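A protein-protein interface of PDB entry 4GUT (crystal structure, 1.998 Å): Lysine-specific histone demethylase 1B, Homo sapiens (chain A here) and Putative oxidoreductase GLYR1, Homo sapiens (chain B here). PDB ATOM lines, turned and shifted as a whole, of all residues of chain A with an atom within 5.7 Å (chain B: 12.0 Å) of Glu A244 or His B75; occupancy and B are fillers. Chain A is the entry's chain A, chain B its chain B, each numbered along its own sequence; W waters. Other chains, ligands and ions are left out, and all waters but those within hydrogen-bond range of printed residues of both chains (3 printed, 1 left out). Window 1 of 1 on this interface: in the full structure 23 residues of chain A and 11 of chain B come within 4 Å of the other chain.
Leu A236 touches just these residues of chain B: His B75 and Phe B76. Printed residues of chain B within 4 Å of Val A238: His B75 and Leu B78. Arg A239 touches just one residue of chain B: His B74. No residue of chain B comes within 4 Å of Val A242. Glu A244 touches just these residues of chain B: His B74 (3.95 Å), His B75 (3.6 Å) and Leu B78 (3.7 Å). Of chain B, only Leu B78 (3.7 Å) comes within 4 Å of Leu A245. No residue of chain B comes within 4 Å of Glu A247. Printed residues of chain B within 4 Å of Leu A315: His B75 and Leu B77. His B75 touches just these residues of chain A: Leu A236, Cys A237, Val A238, Glu A244 and Leu A315. Of the printed residues of chain A, Leu B77 touches Asp A246 and Leu A315. Of the printed residues of chain A, Ser B79 touches Asp A246. Of the printed residues of chain A, Thr B81 touches Asp A246. The nearest residue of chain B that does not touch Glu A244 is Ser B79 (4.5 Å). The nearest residue of chain A that does not touch His B75 is Pro A225 (5.6 Å). The nearest printed residue of chain A that does not touch His B74 is Cys A237 (4.7 Å).
Water W2 lies within hydrogen-bond range of OE2 of Glu A244, N of Leu A245 and OG of Ser B79. Water W3 lies within hydrogen-bond range of the backbone NH (N) of Leu A236, the backbone NH (N) of Phe B76 and the backbone carbonyl oxygen (O) of His B74. Water W1 lies within hydrogen-bond range of O of Phe B73 (2.9 Å), N of Cys A237 (3.0 Å), N of Leu A236 (3.1 Å) and O of His B74 (3.4 Å).
The side-chain carboxylate (OD2) of Asp A246 sits at hydrogen-bond distance from the backbone NH (N) of Gln B80, 2.9 Å away. NH2 of Arg A239 lies within hydrogen-bond range of ND1 of His B74, at 3.2 Å. The side-chain hydroxyl of Thr B81 lies within hydrogen-bond range of the side-chain carboxylate of Asp A246 (2.7 Å). OD2 of Asp A246 sits at hydrogen-bond distance from N of Ser B79 (3.4 Å). The backbone NH of Asp A246 lies within hydrogen-bond range of the backbone carbonyl oxygen of Leu B78 (3.1 Å).
The side-chain carboxylate (OE2) of Glu A244 lies within salt-bridge range of the guanidinium group (NH2) of Arg A239 (3.6 Å). OG of Ser B79 sits at hydrogen-bond distance from O of His B75, 2.7 Å away. OE1 of Glu A247 sits at hydrogen-bond distance from N of Glu A244. The backbone carbonyl oxygen of Asp B70 lies within hydrogen-bond range of a ring nitrogen (NE2) of His B74. The backbone NH (N) of Val A238 is in hydrogen-bond range of the backbone carbonyl oxygen (O) of Pro A225. The backbone carbonyl oxygen (O) of Arg A239 lies within hydrogen-bond range of the guanidinium group (NH1) of Arg A265, at 2.9 Å.
Printed residues of chain B that touch a printed residue of chain A: His B74, His B75, Phe B76, Leu B77, Leu B78, Ser B79, Gln B80 and Thr B81. Hydrophobic or aromatic side chains of chain B that line the printed part of chain A: His B74, His B75, Phe B76, Leu B77 and Leu B78. Of the 15 printed residues of chain A, 8 touch a printed residue of chain B. Hydrophobic or aromatic side chains of chain A that line the printed part of chain B: Leu A236, Val A238 and Leu A315.
Among the printed residues, merely in contact across the chains: Leu A236 with His B75, Leu A236 with Phe B76, Cys A237 with His B75, Val A238 with His B75, Val A238 with Leu B78, Glu A244 with His B74, Glu A244 with His B75, Glu A244 with Leu B78, Leu A245 with Leu B78, Asp A246 with Leu B77, Leu A315 with His B75 and Leu A315 with Leu B77.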
ATOM      1  N   PRO A 225       1.551 -17.360  39.205  1.00  0.00           N
ATOM      2  CA  PRO A 225       0.814 -16.614  38.182  1.00  0.00           C
ATOM      3  C   PRO A 225       0.937 -15.088  38.271  1.00  0.00           C
ATOM      4  O   PRO A 225       0.651 -14.398  37.287  1.00  0.00           O
ATOM      5  CB  PRO A 225      -0.633 -17.049  38.416  1.00  0.00           C
ATOM      6  CG  PRO A 225      -0.688 -17.389  39.868  1.00  0.00           C
ATOM      7  CD  PRO A 225       0.638 -18.021  40.165  1.00  0.00           C
ATOM      8  N   LEU A 236       3.937 -16.209  31.070  1.00  0.00           N
ATOM      9  CA  LEU A 236       2.580 -16.476  31.560  1.00  0.00           C
ATOM     10  C   LEU A 236       2.394 -15.957  32.983  1.00  0.00           C
ATOM     11  O   LEU A 236       2.010 -16.691  33.901  1.00  0.00           O
ATOM     12  CB  LEU A 236       2.205 -17.962  31.434  1.00  0.00           C
ATOM     13  CG  LEU A 236       2.420 -18.669  30.084  1.00  0.00           C
ATOM     14  CD1 LEU A 236       1.695 -20.003  30.114  1.00  0.00           C
ATOM     15  CD2 LEU A 236       1.966 -17.840  28.875  1.00  0.00           C
ATOM     16  N   CYS A 237       2.680 -14.674  33.136  1.00  0.00           N
ATOM     17  CA  CYS A 237       2.616 -14.010  34.416  1.00  0.00           C
ATOM     18  C   CYS A 237       1.793 -12.750  34.235  1.00  0.00           C
ATOM     19  O   CYS A 237       1.926 -12.076  33.217  1.00  0.00           O
ATOM     20  CB  CYS A 237       4.023 -13.633  34.819  1.00  0.00           C
ATOM     21  SG  CYS A 237       4.369 -13.793  36.560  1.00  0.00           S
ATOM     22  N   VAL A 238       0.926 -12.442  35.198  1.00  0.00           N
ATOM     23  CA  VAL A 238       0.197 -11.176  35.151  1.00  0.00           C
ATOM     24  C   VAL A 238       0.644 -10.242  36.268  1.00  0.00           C
ATOM     25  O   VAL A 238       1.147 -10.686  37.311  1.00  0.00           O
ATOM     26  CB  VAL A 238      -1.340 -11.354  35.163  1.00  0.00           C
ATOM     27  CG1 VAL A 238      -1.794 -12.164  33.952  1.00  0.00           C
ATOM     28  CG2 VAL A 238      -1.837 -11.989  36.464  1.00  0.00           C
ATOM     29  N   ARG A 239       0.511  -8.946  36.021  1.00  0.00           N
ATOM     30  CA  ARG A 239       0.627  -7.967  37.083  1.00  0.00           C
ATOM     31  C   ARG A 239      -0.734  -7.939  37.782  1.00  0.00           C
ATOM     32  O   ARG A 239      -1.768  -7.801  37.128  1.00  0.00           O
ATOM     33  CB  ARG A 239       0.985  -6.582  36.533  1.00  0.00           C
ATOM     34  CG  ARG A 239       2.382  -6.472  35.941  1.00  0.00           C
ATOM     35  CD  ARG A 239       2.443  -5.365  34.896  1.00  0.00           C
ATOM     36  NE  ARG A 239       1.704  -5.710  33.675  1.00  0.00           N
ATOM     37  CZ  ARG A 239       1.395  -4.854  32.700  1.00  0.00           C
ATOM     38  NH1 ARG A 239       1.752  -3.574  32.779  1.00  0.00           N
ATOM     39  NH2 ARG A 239       0.722  -5.277  31.638  1.00  0.00           N
ATOM     40  N   VAL A 242      -2.201  -4.263  37.389  1.00  0.00           N
ATOM     41  CA  VAL A 242      -2.391  -3.691  36.055  1.00  0.00           C
ATOM     42  C   VAL A 242      -3.183  -4.636  35.156  1.00  0.00           C
ATOM     43  O   VAL A 242      -2.887  -5.830  35.093  1.00  0.00           O
ATOM     44  CB  VAL A 242      -1.038  -3.346  35.379  1.00  0.00           C
ATOM     45  CG1 VAL A 242      -1.261  -2.575  34.082  1.00  0.00           C
ATOM     46  CG2 VAL A 242      -0.148  -2.545  36.318  1.00  0.00           C
ATOM     47  N   MET A 243      -4.188  -4.100  34.471  1.00  0.00           N
ATOM     48  CA  MET A 243      -4.931  -4.861  33.472  1.00  0.00           C
ATOM     49  C   MET A 243      -4.082  -5.059  32.217  1.00  0.00           C
ATOM     50  O   MET A 243      -3.333  -4.165  31.822  1.00  0.00           O
ATOM     51  CB  MET A 243      -6.245  -4.166  33.114  1.00  0.00           C
ATOM     52  CG  MET A 243      -7.311  -4.246  34.208  1.00  0.00           C
ATOM     53  SD  MET A 243      -8.831  -3.347  33.861  1.00  0.00           S
ATOM     54  CE  MET A 243      -9.688  -4.437  32.723  1.00  0.00           C
ATOM     55  N   GLU A 244      -4.198  -6.235  31.606  1.00  0.00           N
ATOM     56  CA  GLU A 244      -3.464  -6.557  30.380  1.00  0.00           C
ATOM     57  C   GLU A 244      -4.207  -5.994  29.187  1.00  0.00           C
ATOM     58  O   GLU A 244      -5.382  -5.649  29.293  1.00  0.00           O
ATOM     59  CB  GLU A 244      -3.323  -8.074  30.219  1.00  0.00           C
ATOM     60  CG  GLU A 244      -2.628  -8.769  31.379  1.00  0.00           C
ATOM     61  CD  GLU A 244      -1.115  -8.729  31.285  1.00  0.00           C
ATOM     62  OE1 GLU A 244      -0.461  -9.130  32.265  1.00  0.00           O
ATOM     63  OE2 GLU A 244      -0.569  -8.312  30.241  1.00  0.00           O
ATOM     64  N   LEU A 245      -3.527  -5.932  28.044  1.00  0.00           N
ATOM     65  CA  LEU A 245      -4.104  -5.376  26.822  1.00  0.00           C
ATOM     66  C   LEU A 245      -5.441  -5.995  26.442  1.00  0.00           C
ATOM     67  O   LEU A 245      -6.409  -5.279  26.200  1.00  0.00           O
ATOM     68  CB  LEU A 245      -3.107  -5.473  25.654  1.00  0.00           C
ATOM     69  CG  LEU A 245      -1.863  -4.572  25.761  1.00  0.00           C
ATOM     70  CD1 LEU A 245      -1.038  -4.596  24.477  1.00  0.00           C
ATOM     71  CD2 LEU A 245      -2.258  -3.139  26.107  1.00  0.00           C
ATOM     72  N   ASP A 246      -5.512  -7.322  26.413  1.00  0.00           N
ATOM     73  CA  ASP A 246      -6.753  -7.998  26.024  1.00  0.00           C
ATOM     74  C   ASP A 246      -7.855  -7.761  27.054  1.00  0.00           C
ATOM     75  O   ASP A 246      -9.032  -7.746  26.714  1.00  0.00           O
ATOM     76  CB  ASP A 246      -6.538  -9.504  25.833  1.00  0.00           C
ATOM     77  CG  ASP A 246      -5.626  -9.834  24.648  1.00  0.00           C
ATOM     78  OD1 ASP A 246      -5.058  -8.909  24.016  1.00  0.00           O
ATOM     79  OD2 ASP A 246      -5.465 -11.042  24.365  1.00  0.00           O
ATOM     80  N   GLU A 247      -7.459  -7.582  28.310  1.00  0.00           N
ATOM     81  CA  GLU A 247      -8.420  -7.293  29.379  1.00  0.00           C
ATOM     82  C   GLU A 247      -9.041  -5.902  29.178  1.00  0.00           C
ATOM     83  O   GLU A 247     -10.273  -5.755  29.178  1.00  0.00           O
ATOM     84  CB  GLU A 247      -7.747  -7.422  30.749  1.00  0.00           C
ATOM     85  CG  GLU A 247      -7.226  -8.825  31.032  1.00  0.00           C
ATOM     86  CD  GLU A 247      -6.656  -8.976  32.425  1.00  0.00           C
ATOM     87  OE1 GLU A 247      -5.720  -8.222  32.774  1.00  0.00           O
ATOM     88  OE2 GLU A 247      -7.140  -9.865  33.169  1.00  0.00           O
ATOM     89  N   LEU A 248      -8.188  -4.900  28.970  1.00  0.00           N
ATOM     90  CA  LEU A 248      -8.640  -3.543  28.621  1.00  0.00           C
ATOM     91  C   LEU A 248      -9.550  -3.540  27.403  1.00  0.00           C
ATOM     92  O   LEU A 248     -10.544  -2.815  27.364  1.00  0.00           O
ATOM     93  CB  LEU A 248      -7.453  -2.612  28.361  1.00  0.00           C
ATOM     94  CG  LEU A 248      -6.834  -1.750  29.470  1.00  0.00           C
ATOM     95  CD1 LEU A 248      -7.766  -1.587  30.665  1.00  0.00           C
ATOM     96  CD2 LEU A 248      -5.476  -2.285  29.899  1.00  0.00           C
ATOM     97  N   TYR A 249      -9.209  -4.370  26.417  1.00  0.00           N
ATOM     98  CA  TYR A 249      -9.962  -4.471  25.175  1.00  0.00           C
ATOM     99  C   TYR A 249     -11.385  -5.001  25.392  1.00  0.00           C
ATOM    100  O   TYR A 249     -12.336  -4.502  24.789  1.00  0.00           O
ATOM    101  CB  TYR A 249      -9.197  -5.338  24.165  1.00  0.00           C
ATOM    102  CG  TYR A 249      -9.908  -5.528  22.842  1.00  0.00           C
ATOM    103  CD1 TYR A 249      -9.758  -4.600  21.805  1.00  0.00           C
ATOM    104  CD2 TYR A 249     -10.735  -6.632  22.624  1.00  0.00           C
ATOM    105  CE1 TYR A 249     -10.415  -4.767  20.593  1.00  0.00           C
ATOM    106  CE2 TYR A 249     -11.396  -6.808  21.415  1.00  0.00           C
ATOM    107  CZ  TYR A 249     -11.234  -5.877  20.403  1.00  0.00           C
ATOM    108  OH  TYR A 249     -11.890  -6.059  19.204  1.00  0.00           O
ATOM    109  N   ARG A 265     -10.472 -10.806  39.026  1.00  0.00           N
ATOM    110  CA  ARG A 265      -9.546 -11.576  38.191  1.00  0.00           C
ATOM    111  C   ARG A 265      -8.493 -12.304  39.035  1.00  0.00           C
ATOM    112  O   ARG A 265      -8.231 -13.490  38.810  1.00  0.00           O
ATOM    113  CB  ARG A 265      -8.888 -10.699  37.110  1.00  0.00           C
ATOM    114  CG  ARG A 265      -7.852 -11.445  36.271  1.00  0.00           C
ATOM    115  CD  ARG A 265      -6.441 -11.078  36.702  1.00  0.00           C
ATOM    116  NE  ARG A 265      -5.956  -9.963  35.886  1.00  0.00           N
ATOM    117  CZ  ARG A 265      -4.926  -9.183  36.191  1.00  0.00           C
ATOM    118  NH1 ARG A 265      -4.256  -9.351  37.326  1.00  0.00           N
ATOM    119  NH2 ARG A 265      -4.559  -8.234  35.339  1.00  0.00           N
ATOM    120  N   LEU A 315      -6.734 -19.082  30.610  1.00  0.00           N
ATOM    121  CA  LEU A 315      -6.010 -18.833  31.864  1.00  0.00           C
ATOM    122  C   LEU A 315      -6.486 -19.772  32.977  1.00  0.00           C
ATOM    123  O   LEU A 315      -5.737 -20.088  33.900  1.00  0.00           O
ATOM    124  CB  LEU A 315      -6.164 -17.372  32.302  1.00  0.00           C
ATOM    125  CG  LEU A 315      -5.506 -16.182  31.568  1.00  0.00           C
ATOM    126  CD1 LEU A 315      -4.127 -15.878  32.135  1.00  0.00           C
ATOM    127  CD2 LEU A 315      -5.438 -16.308  30.055  1.00  0.00           C
ATOM    128  N   ASP B  70       6.047  -2.722  27.513  1.00  0.00           N
ATOM    129  CA  ASP B  70       7.137  -3.555  26.922  1.00  0.00           C
ATOM    130  C   ASP B  70       6.740  -5.032  26.809  1.00  0.00           C
ATOM    131  O   ASP B  70       6.228  -5.614  27.771  1.00  0.00           O
ATOM    132  CB  ASP B  70       8.448  -3.394  27.710  1.00  0.00           C
ATOM    133  CG  ASP B  70       8.276  -3.604  29.214  1.00  0.00           C
ATOM    134  OD1 ASP B  70       7.136  -3.802  29.692  1.00  0.00           O
ATOM    135  OD2 ASP B  70       9.301  -3.563  29.926  1.00  0.00           O
ATOM    136  N   PRO B  71       6.976  -5.642  25.628  1.00  0.00           N
ATOM    137  CA  PRO B  71       6.615  -7.041  25.363  1.00  0.00           C
ATOM    138  C   PRO B  71       7.507  -8.064  26.076  1.00  0.00           C
ATOM    139  O   PRO B  71       7.269  -9.267  25.962  1.00  0.00           O
ATOM    140  CB  PRO B  71       6.773  -7.169  23.838  1.00  0.00           C
ATOM    141  CG  PRO B  71       6.905  -5.771  23.320  1.00  0.00           C
ATOM    142  CD  PRO B  71       7.547  -5.001  24.431  1.00  0.00           C
ATOM    143  N   HIS B  72       8.517  -7.583  26.804  1.00  0.00           N
ATOM    144  CA  HIS B  72       9.400  -8.437  27.607  1.00  0.00           C
ATOM    145  C   HIS B  72       8.714  -8.957  28.845  1.00  0.00           C
ATOM    146  O   HIS B  72       9.301  -9.739  29.602  1.00  0.00           O
ATOM    147  CB  HIS B  72      10.648  -7.668  28.043  1.00  0.00           C
ATOM    148  CG  HIS B  72      11.311  -6.878  26.940  1.00  0.00           C
ATOM    149  ND1 HIS B  72      12.360  -7.350  26.244  1.00  0.00           N
ATOM    150  CD2 HIS B  72      11.049  -5.601  26.441  1.00  0.00           C
ATOM    151  CE1 HIS B  72      12.750  -6.429  25.344  1.00  0.00           C
ATOM    152  NE2 HIS B  72      11.944  -5.360  25.464  1.00  0.00           N
ATOM    153  N   PHE B  73       7.475  -8.514  29.067  1.00  0.00           N
ATOM    154  CA  PHE B  73       6.749  -8.765  30.315  1.00  0.00           C
ATOM    155  C   PHE B  73       5.366  -9.392  30.110  1.00  0.00           C
ATOM    156  O   PHE B  73       4.982 -10.316  30.838  1.00  0.00           O
ATOM    157  CB  PHE B  73       6.600  -7.456  31.112  1.00  0.00           C
ATOM    158  CG  PHE B  73       7.814  -7.093  31.928  1.00  0.00           C
ATOM    159  CD1 PHE B  73       7.847  -7.344  33.298  1.00  0.00           C
ATOM    160  CD2 PHE B  73       8.925  -6.492  31.333  1.00  0.00           C
ATOM    161  CE1 PHE B  73       8.962  -7.009  34.055  1.00  0.00           C
ATOM    162  CE2 PHE B  73      10.044  -6.157  32.087  1.00  0.00           C
ATOM    163  CZ  PHE B  73      10.062  -6.416  33.449  1.00  0.00           C
ATOM    164  N   HIS B  74       4.634  -8.887  29.117  1.00  0.00           N
ATOM    165  CA  HIS B  74       3.200  -9.148  28.985  1.00  0.00           C
ATOM    166  C   HIS B  74       2.825 -10.593  28.797  1.00  0.00           C
ATOM    167  O   HIS B  74       3.545 -11.365  28.156  1.00  0.00           O
ATOM    168  CB  HIS B  74       2.594  -8.299  27.873  1.00  0.00           C
ATOM    169  CG  HIS B  74       2.795  -6.811  28.059  1.00  0.00           C
ATOM    170  ND1 HIS B  74       2.718  -6.210  29.267  1.00  0.00           N
ATOM    171  CD2 HIS B  74       3.063  -5.801  27.133  1.00  0.00           C
ATOM    172  CE1 HIS B  74       2.937  -4.889  29.123  1.00  0.00           C
ATOM    173  NE2 HIS B  74       3.147  -4.640  27.818  1.00  0.00           N
ATOM    174  N   HIS B  75       1.678 -10.955  29.364  1.00  0.00           N
ATOM    175  CA  HIS B  75       1.156 -12.309  29.300  1.00  0.00           C
ATOM    176  C   HIS B  75       0.801 -12.678  27.890  1.00  0.00           C
ATOM    177  O   HIS B  75      -0.025 -12.024  27.243  1.00  0.00           O
ATOM    178  CB  HIS B  75      -0.054 -12.437  30.216  1.00  0.00           C
ATOM    179  CG  HIS B  75      -0.429 -13.860  30.549  1.00  0.00           C
ATOM    180  ND1 HIS B  75      -0.900 -14.721  29.628  1.00  0.00           N
ATOM    181  CD2 HIS B  75      -0.424 -14.546  31.766  1.00  0.00           C
ATOM    182  CE1 HIS B  75      -1.161 -15.907  30.217  1.00  0.00           C
ATOM    183  NE2 HIS B  75      -0.874 -15.793  31.526  1.00  0.00           N
ATOM    184  N   PHE B  76       1.424 -13.749  27.408  1.00  0.00           N
ATOM    185  CA  PHE B  76       1.213 -14.252  26.049  1.00  0.00           C
ATOM    186  C   PHE B  76      -0.260 -14.448  25.675  1.00  0.00           C
ATOM    187  O   PHE B  76      -0.672 -14.102  24.561  1.00  0.00           O
ATOM    188  CB  PHE B  76       2.016 -15.544  25.840  1.00  0.00           C
ATOM    189  CG  PHE B  76       1.692 -16.275  24.560  1.00  0.00           C
ATOM    190  CD1 PHE B  76       2.297 -15.913  23.360  1.00  0.00           C
ATOM    191  CD2 PHE B  76       0.795 -17.342  24.557  1.00  0.00           C
ATOM    192  CE1 PHE B  76       2.000 -16.587  22.180  1.00  0.00           C
ATOM    193  CE2 PHE B  76       0.499 -18.018  23.381  1.00  0.00           C
ATOM    194  CZ  PHE B  76       1.104 -17.639  22.189  1.00  0.00           C
ATOM    195  N   LEU B  77      -1.056 -15.001  26.590  1.00  0.00           N
ATOM    196  CA  LEU B  77      -2.460 -15.265  26.284  1.00  0.00           C
ATOM    197  C   LEU B  77      -3.356 -14.018  26.407  1.00  0.00           C
ATOM    198  O   LEU B  77      -4.479 -14.021  25.919  1.00  0.00           O
ATOM    199  CB  LEU B  77      -3.005 -16.429  27.127  1.00  0.00           C
ATOM    200  CG  LEU B  77      -2.467 -17.859  26.898  1.00  0.00           C
ATOM    201  CD1 LEU B  77      -3.128 -18.837  27.869  1.00  0.00           C
ATOM    202  CD2 LEU B  77      -2.665 -18.338  25.460  1.00  0.00           C
ATOM    203  N   LEU B  78      -2.852 -12.956  27.026  1.00  0.00           N
ATOM    204  CA  LEU B  78      -3.623 -11.715  27.163  1.00  0.00           C
ATOM    205  C   LEU B  78      -3.008 -10.547  26.381  1.00  0.00           C
ATOM    206  O   LEU B  78      -3.259  -9.376  26.686  1.00  0.00           O
ATOM    207  CB  LEU B  78      -3.797 -11.344  28.640  1.00  0.00           C
ATOM    208  CG  LEU B  78      -4.587 -12.349  29.497  1.00  0.00           C
ATOM    209  CD1 LEU B  78      -4.438 -12.022  30.974  1.00  0.00           C
ATOM    210  CD2 LEU B  78      -6.044 -12.391  29.074  1.00  0.00           C
ATOM    211  N   SER B  79      -2.219 -10.880  25.360  1.00  0.00           N
ATOM    212  CA  SER B  79      -1.615  -9.880  24.485  1.00  0.00           C
ATOM    213  C   SER B  79      -1.922 -10.188  23.027  1.00  0.00           C
ATOM    214  O   SER B  79      -1.152  -9.830  22.147  1.00  0.00           O
ATOM    215  CB  SER B  79      -0.097  -9.839  24.692  1.00  0.00           C
ATOM    216  OG  SER B  79       0.226  -9.592  26.046  1.00  0.00           O
ATOM    217  N   GLN B  80      -3.054 -10.837  22.773  1.00  0.00           N
ATOM    218  CA  GLN B  80      -3.382 -11.299  21.430  1.00  0.00           C
ATOM    219  C   GLN B  80      -4.143 -10.289  20.557  1.00  0.00           C
ATOM    220  O   GLN B  80      -4.468 -10.598  19.404  1.00  0.00           O
ATOM    221  CB  GLN B  80      -4.114 -12.648  21.481  1.00  0.00           C
ATOM    222  CG  GLN B  80      -3.284 -13.784  22.075  1.00  0.00           C
ATOM    223  CD  GLN B  80      -2.055 -14.122  21.248  1.00  0.00           C
ATOM    224  OE1 GLN B  80      -2.062 -13.988  20.029  1.00  0.00           O
ATOM    225  NE2 GLN B  80      -0.996 -14.580  21.912  1.00  0.00           N
ATOM    226  N   THR B  81      -4.409  -9.091  21.088  1.00  0.00           N
ATOM    227  CA  THR B  81      -5.062  -8.026  20.299  1.00  0.00           C
ATOM    228  C   THR B  81      -4.099  -6.910  19.887  1.00  0.00           C
ATOM    229  O   THR B  81      -2.921  -6.910  20.262  1.00  0.00           O
ATOM    230  CB  THR B  81      -6.279  -7.403  21.027  1.00  0.00           C
ATOM    231  OG1 THR B  81      -5.886  -6.943  22.328  1.00  0.00           O
ATOM    232  CG2 THR B  81      -7.422  -8.418  21.158  1.00  0.00           C
HETATM  233  O   HOH W   1       4.190 -13.124  31.050  1.00  0.00           O
HETATM  234  O   HOH W   2      -0.846  -7.034  27.899  1.00  0.00           O
HETATM  235  O   HOH W   3       4.115 -14.755  28.722  1.00  0.00           O
